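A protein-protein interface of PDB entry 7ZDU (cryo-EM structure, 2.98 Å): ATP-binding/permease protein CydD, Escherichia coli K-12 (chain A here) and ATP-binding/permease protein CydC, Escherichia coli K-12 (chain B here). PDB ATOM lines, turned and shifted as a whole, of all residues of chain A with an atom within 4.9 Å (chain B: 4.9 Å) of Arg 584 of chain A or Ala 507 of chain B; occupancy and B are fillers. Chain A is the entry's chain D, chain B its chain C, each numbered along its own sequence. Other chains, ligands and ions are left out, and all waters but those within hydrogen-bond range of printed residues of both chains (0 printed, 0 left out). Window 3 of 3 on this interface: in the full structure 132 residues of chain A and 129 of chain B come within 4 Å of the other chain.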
ATOM      1  N   HIS A 542      -7.022  32.974   7.556  1.00  0.00           N
ATOM      2  CA  HIS A 542      -7.737  31.733   7.794  1.00  0.00           C
ATOM      3  C   HIS A 542      -7.958  30.911   6.535  1.00  0.00           C
ATOM      4  O   HIS A 542      -8.445  29.780   6.637  1.00  0.00           O
ATOM      5  CB  HIS A 542      -9.095  32.017   8.455  1.00  0.00           C
ATOM      6  CG  HIS A 542      -8.988  32.459   9.881  1.00  0.00           C
ATOM      7  ND1 HIS A 542      -9.452  33.680  10.319  1.00  0.00           N
ATOM      8  CD2 HIS A 542      -8.467  31.842  10.968  1.00  0.00           C
ATOM      9  CE1 HIS A 542      -9.223  33.797  11.614  1.00  0.00           C
ATOM     10  NE2 HIS A 542      -8.626  32.695  12.032  1.00  0.00           N
ATOM     11  N   GLN A 543      -7.621  31.438   5.358  1.00  0.00           N
ATOM     12  CA  GLN A 543      -7.695  30.677   4.111  1.00  0.00           C
ATOM     13  C   GLN A 543      -6.513  29.709   4.022  1.00  0.00           C
ATOM     14  O   GLN A 543      -5.492  29.970   3.388  1.00  0.00           O
ATOM     15  CB  GLN A 543      -7.740  31.613   2.910  1.00  0.00           C
ATOM     16  CG  GLN A 543      -9.053  32.353   2.717  1.00  0.00           C
ATOM     17  CD  GLN A 543      -9.307  33.398   3.782  1.00  0.00           C
ATOM     18  OE1 GLN A 543     -10.296  33.329   4.511  1.00  0.00           O
ATOM     19  NE2 GLN A 543      -8.414  34.374   3.878  1.00  0.00           N
ATOM     20  N   LEU A 544      -6.676  28.569   4.687  1.00  0.00           N
ATOM     21  CA  LEU A 544      -5.619  27.574   4.800  1.00  0.00           C
ATOM     22  C   LEU A 544      -5.262  26.956   3.455  1.00  0.00           C
ATOM     23  O   LEU A 544      -4.157  26.432   3.281  1.00  0.00           O
ATOM     24  CB  LEU A 544      -6.042  26.481   5.779  1.00  0.00           C
ATOM     25  CG  LEU A 544      -6.348  26.976   7.191  1.00  0.00           C
ATOM     26  CD1 LEU A 544      -6.898  25.857   8.060  1.00  0.00           C
ATOM     27  CD2 LEU A 544      -5.107  27.581   7.807  1.00  0.00           C
ATOM     28  N   GLU A 545      -6.188  27.010   2.497  1.00  0.00           N
ATOM     29  CA  GLU A 545      -5.997  26.288   1.242  1.00  0.00           C
ATOM     30  C   GLU A 545      -4.945  26.948   0.357  1.00  0.00           C
ATOM     31  O   GLU A 545      -4.079  26.266  -0.204  1.00  0.00           O
ATOM     32  CB  GLU A 545      -7.328  26.179   0.500  1.00  0.00           C
ATOM     33  CG  GLU A 545      -8.469  25.620   1.339  1.00  0.00           C
ATOM     34  CD  GLU A 545      -9.834  25.906   0.740  1.00  0.00           C
ATOM     35  OE1 GLU A 545     -10.797  25.192   1.089  1.00  0.00           O
ATOM     36  OE2 GLU A 545      -9.947  26.845  -0.076  1.00  0.00           O
ATOM     37  N   LEU A 580      -7.316  21.215  11.809  1.00  0.00           N
ATOM     38  CA  LEU A 580      -7.884  22.539  11.583  1.00  0.00           C
ATOM     39  C   LEU A 580      -8.279  22.723  10.125  1.00  0.00           C
ATOM     40  O   LEU A 580      -9.319  23.319   9.825  1.00  0.00           O
ATOM     41  CB  LEU A 580      -6.890  23.616  12.017  1.00  0.00           C
ATOM     42  CG  LEU A 580      -7.404  25.052  12.017  1.00  0.00           C
ATOM     43  CD1 LEU A 580      -8.572  25.188  12.974  1.00  0.00           C
ATOM     44  CD2 LEU A 580      -6.288  25.996  12.405  1.00  0.00           C
ATOM     45  N   LEU A 581      -7.458  22.219   9.202  1.00  0.00           N
ATOM     46  CA  LEU A 581      -7.812  22.254   7.789  1.00  0.00           C
ATOM     47  C   LEU A 581      -8.919  21.265   7.454  1.00  0.00           C
ATOM     48  O   LEU A 581      -9.619  21.453   6.454  1.00  0.00           O
ATOM     49  CB  LEU A 581      -6.568  21.978   6.937  1.00  0.00           C
ATOM     50  CG  LEU A 581      -6.610  22.192   5.421  1.00  0.00           C
ATOM     51  CD1 LEU A 581      -5.242  22.621   4.928  1.00  0.00           C
ATOM     52  CD2 LEU A 581      -7.046  20.932   4.691  1.00  0.00           C
ATOM     53  N   ALA A 582      -9.097  20.223   8.271  1.00  0.00           N
ATOM     54  CA  ALA A 582     -10.116  19.218   7.987  1.00  0.00           C
ATOM     55  C   ALA A 582     -11.517  19.815   8.033  1.00  0.00           C
ATOM     56  O   ALA A 582     -12.355  19.506   7.178  1.00  0.00           O
ATOM     57  CB  ALA A 582      -9.995  18.056   8.971  1.00  0.00           C
ATOM     58  N   HIS A 583     -11.794  20.666   9.023  1.00  0.00           N
ATOM     59  CA  HIS A 583     -13.103  21.309   9.088  1.00  0.00           C
ATOM     60  C   HIS A 583     -13.301  22.284   7.936  1.00  0.00           C
ATOM     61  O   HIS A 583     -14.442  22.586   7.569  1.00  0.00           O
ATOM     62  CB  HIS A 583     -13.278  22.014  10.431  1.00  0.00           C
ATOM     63  CG  HIS A 583     -13.175  21.096  11.609  1.00  0.00           C
ATOM     64  ND1 HIS A 583     -11.993  20.492  11.980  1.00  0.00           N
ATOM     65  CD2 HIS A 583     -14.108  20.669  12.491  1.00  0.00           C
ATOM     66  CE1 HIS A 583     -12.201  19.738  13.045  1.00  0.00           C
ATOM     67  NE2 HIS A 583     -13.476  19.827  13.375  1.00  0.00           N
ATOM     68  N   ARG A 584     -12.213  22.787   7.364  1.00  0.00           N
ATOM     69  CA  ARG A 584     -12.281  23.536   6.122  1.00  0.00           C
ATOM     70  C   ARG A 584     -12.393  22.570   4.944  1.00  0.00           C
ATOM     71  O   ARG A 584     -12.071  21.384   5.050  1.00  0.00           O
ATOM     72  CB  ARG A 584     -11.048  24.429   5.967  1.00  0.00           C
ATOM     73  CG  ARG A 584     -11.178  25.511   4.911  1.00  0.00           C
ATOM     74  CD  ARG A 584     -10.063  26.535   5.014  1.00  0.00           C
ATOM     75  NE  ARG A 584     -10.179  27.553   3.976  1.00  0.00           N
ATOM     76  CZ  ARG A 584     -10.948  28.631   4.073  1.00  0.00           C
ATOM     77  NH1 ARG A 584     -10.997  29.506   3.078  1.00  0.00           N
ATOM     78  NH2 ARG A 584     -11.668  28.836   5.167  1.00  0.00           N
ATOM     79  N   GLN A 585     -12.866  23.094   3.814  1.00  0.00           N
ATOM     80  CA  GLN A 585     -12.991  22.326   2.575  1.00  0.00           C
ATOM     81  C   GLN A 585     -13.907  21.115   2.776  1.00  0.00           C
ATOM     82  O   GLN A 585     -13.492  19.957   2.700  1.00  0.00           O
ATOM     83  CB  GLN A 585     -11.609  21.908   2.056  1.00  0.00           C
ATOM     84  CG  GLN A 585     -11.604  21.283   0.669  1.00  0.00           C
ATOM     85  CD  GLN A 585     -10.214  20.873   0.227  1.00  0.00           C
ATOM     86  OE1 GLN A 585      -9.822  21.097  -0.919  1.00  0.00           O
ATOM     87  NE2 GLN A 585      -9.457  20.272   1.137  1.00  0.00           N
ATOM     88  N   GLU A 586     -15.172  21.409   3.063  1.00  0.00           N
ATOM     89  CA  GLU A 586     -16.185  20.370   3.200  1.00  0.00           C
ATOM     90  C   GLU A 586     -17.289  20.547   2.162  1.00  0.00           C
ATOM     91  O   GLU A 586     -18.350  21.096   2.457  1.00  0.00           O
ATOM     92  CB  GLU A 586     -16.785  20.379   4.608  1.00  0.00           C
ATOM     93  CG  GLU A 586     -15.884  19.793   5.679  1.00  0.00           C
ATOM     94  CD  GLU A 586     -16.588  19.660   7.016  1.00  0.00           C
ATOM     95  OE1 GLU A 586     -17.730  20.148   7.139  1.00  0.00           O
ATOM     96  OE2 GLU A 586     -16.000  19.065   7.944  1.00  0.00           O
ATOM     97  N   LEU B 505     -13.846  34.011  11.644  1.00  0.00           N
ATOM     98  CA  LEU B 505     -13.742  32.795  12.435  1.00  0.00           C
ATOM     99  C   LEU B 505     -12.984  31.740  11.645  1.00  0.00           C
ATOM    100  O   LEU B 505     -13.086  31.678  10.416  1.00  0.00           O
ATOM    101  CB  LEU B 505     -15.125  32.264  12.814  1.00  0.00           C
ATOM    102  CG  LEU B 505     -16.066  33.217  13.548  1.00  0.00           C
ATOM    103  CD1 LEU B 505     -17.308  32.482  14.012  1.00  0.00           C
ATOM    104  CD2 LEU B 505     -15.358  33.859  14.719  1.00  0.00           C
ATOM    105  N   ASP B 506     -12.222  30.912  12.353  1.00  0.00           N
ATOM    106  CA  ASP B 506     -11.485  29.842  11.702  1.00  0.00           C
ATOM    107  C   ASP B 506     -12.441  28.742  11.250  1.00  0.00           C
ATOM    108  O   ASP B 506     -13.656  28.813  11.445  1.00  0.00           O
ATOM    109  CB  ASP B 506     -10.423  29.284  12.641  1.00  0.00           C
ATOM    110  CG  ASP B 506     -10.971  28.988  14.011  1.00  0.00           C
ATOM    111  OD1 ASP B 506     -11.871  29.726  14.458  1.00  0.00           O
ATOM    112  OD2 ASP B 506     -10.520  28.007  14.631  1.00  0.00           O
ATOM    113  N   ALA B 507     -11.875  27.703  10.635  1.00  0.00           N
ATOM    114  CA  ALA B 507     -12.694  26.615  10.113  1.00  0.00           C
ATOM    115  C   ALA B 507     -13.428  25.879  11.227  1.00  0.00           C
ATOM    116  O   ALA B 507     -14.610  25.548  11.087  1.00  0.00           O
ATOM    117  CB  ALA B 507     -11.827  25.645   9.313  1.00  0.00           C
ATOM    118  N   THR B 508     -12.743  25.611  12.339  1.00  0.00           N
ATOM    119  CA  THR B 508     -13.344  24.814  13.404  1.00  0.00           C
ATOM    120  C   THR B 508     -14.473  25.568  14.096  1.00  0.00           C
ATOM    121  O   THR B 508     -15.568  25.026  14.287  1.00  0.00           O
ATOM    122  CB  THR B 508     -12.278  24.402  14.416  1.00  0.00           C
ATOM    123  OG1 THR B 508     -11.360  23.490  13.801  1.00  0.00           O
ATOM    124  CG2 THR B 508     -12.920  23.730  15.616  1.00  0.00           C
ATOM    125  N   THR B 509     -14.227  26.821  14.484  1.00  0.00           N
ATOM    126  CA  THR B 509     -15.245  27.585  15.196  1.00  0.00           C
ATOM    127  C   THR B 509     -16.436  27.895  14.300  1.00  0.00           C
ATOM    128  O   THR B 509     -17.586  27.854  14.751  1.00  0.00           O
ATOM    129  CB  THR B 509     -14.645  28.875  15.753  1.00  0.00           C
ATOM    130  OG1 THR B 509     -13.610  28.555  16.689  1.00  0.00           O
ATOM    131  CG2 THR B 509     -15.706  29.696  16.456  1.00  0.00           C
ATOM    132  N   GLU B 510     -16.182  28.209  13.028  1.00  0.00           N
ATOM    133  CA  GLU B 510     -17.272  28.534  12.116  1.00  0.00           C
ATOM    134  C   GLU B 510     -18.221  27.357  11.947  1.00  0.00           C
ATOM    135  O   GLU B 510     -19.445  27.527  11.979  1.00  0.00           O
ATOM    136  CB  GLU B 510     -16.710  28.973  10.766  1.00  0.00           C
ATOM    137  CG  GLU B 510     -17.724  28.993   9.647  1.00  0.00           C
ATOM    138  CD  GLU B 510     -17.113  29.399   8.324  1.00  0.00           C
ATOM    139  OE1 GLU B 510     -15.881  29.599   8.273  1.00  0.00           O
ATOM    140  OE2 GLU B 510     -17.862  29.518   7.333  1.00  0.00           O
ATOM    141  N   SER B 511     -17.677  26.150  11.775  1.00  0.00           N
ATOM    142  CA  SER B 511     -18.522  24.963  11.718  1.00  0.00           C
ATOM    143  C   SER B 511     -19.253  24.752  13.036  1.00  0.00           C
ATOM    144  O   SER B 511     -20.415  24.329  13.052  1.00  0.00           O
ATOM    145  CB  SER B 511     -17.684  23.737  11.368  1.00  0.00           C
ATOM    146  OG  SER B 511     -16.838  23.381  12.446  1.00  0.00           O
ATOM    147  N   ARG B 532     -18.968  32.901   1.728  1.00  0.00           N
ATOM    148  CA  ARG B 532     -18.381  31.569   1.713  1.00  0.00           C
ATOM    149  C   ARG B 532     -19.385  30.578   1.141  1.00  0.00           C
ATOM    150  O   ARG B 532     -20.520  30.491   1.621  1.00  0.00           O
ATOM    151  CB  ARG B 532     -17.958  31.142   3.120  1.00  0.00           C
ATOM    152  CG  ARG B 532     -17.254  29.798   3.164  1.00  0.00           C
ATOM    153  CD  ARG B 532     -16.165  29.771   4.222  1.00  0.00           C
ATOM    154  NE  ARG B 532     -15.266  28.636   4.034  1.00  0.00           N
ATOM    155  CZ  ARG B 532     -15.058  27.687   4.939  1.00  0.00           C
ATOM    156  NH1 ARG B 532     -15.684  27.730   6.107  1.00  0.00           N
ATOM    157  NH2 ARG B 532     -14.224  26.692   4.677  1.00  0.00           N
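His 542 of chain A touches Asp 506 of chain B (CD2 to CB, 3.6 Å). Asp 506 of chain B touches Leu 580 of chain A. Leu 580 of chain A touches Ala 507 of chain B (O to CB, 3.5 Å). Leu 580 of chain A touches Thr 508 of chain B (CD1 to OG1, 3.4 Å). Ala 507 of chain B touches His 583 of chain A (O to CB, 3.8 Å). Thr 508 of chain B touches His 583 of chain A. CD2 of His 583 of chain A touches OG of Ser 511 of chain B, at 3.8 Å. Arg 584 of chain A touches Ala 507 of chain B (N to CB, 3.5 Å). N of Gln 585 of chain A touches NH2 of Arg 532 of chain B (3.9 Å).
Of the printed residues of chain B, His 542 of chain A touches Asp 506. Printed residues of chain B within 4 Å of Arg 584 of chain A: Ala 507 (3.5 Å) and Arg 532 (3.3 Å). Printed residues of chain B within 4 Å of Gln 585 of chain A: Arg 532. Ala 507 of chain B touches just these residues of chain A: Leu 580 (3.5 Å), His 583 (3.8 Å) and Arg 584 (3.5 Å). Of the printed residues of chain A, Thr 508 of chain B touches Leu 580 (3.4 Å) and His 583 (3.6 Å). Printed residues of chain A within 4 Å of Ser 511 of chain B: His 583. The nearest printed residue of chain B that does not touch Arg 584 of chain A is Glu 510 of chain B (5.3 Å). The nearest printed residue of chain A that does not touch Ala 507 of chain B is Leu 544 of chain A (5.1 Å). The nearest printed residue of chain B that does not touch His 542 of chain A is Leu 505 of chain B (4.2 Å).
The guanidinium group (NH2) of Arg 532 of chain B lies close to the guanidinium group (NH2) of Arg 584 of chain A, 3.4 Å away.
Hydrophobic or aromatic side chains of chain B within 4 Å of the printed part of chain A: Ala 507. Of the 11 printed residues of chain A, 5 touch a printed residue of chain B. Hydrophobic or aromatic side chains of chain A within 4 Å of the printed part of chain B: His 542, Leu 580 and His 583. Among the printed residues, 10 pairs touch across the chains.
The side-chain carboxylate (OD1) of Asp 506 of chain B sits at hydrogen-bond distance from the side-chain hydroxyl (OG1) of Thr 509 of chain B. The backbone carbonyl oxygen (O) of Ala 507 of chain B lies within hydrogen-bond range of the side-chain hydroxyl (OG) of Ser 511 of chain B (3.4 Å). The side-chain hydroxyl (OG) of Ser 511 of chain B lies within hydrogen-bond range of the backbone carbonyl oxygen (O) of Thr 508 of chain B, at 2.8 Å. The side-chain carboxylate (OE1) of Glu 510 of chain B is in salt-bridge range of the guanidinium group (NH1) of Arg 532 of chain B, 2.9 Å away. The side-chain carboxylate (OE1) of Glu 545 of chain A lies within salt-bridge range of the guanidinium group (NE) of Arg 584 of chain A (3.8 Å).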
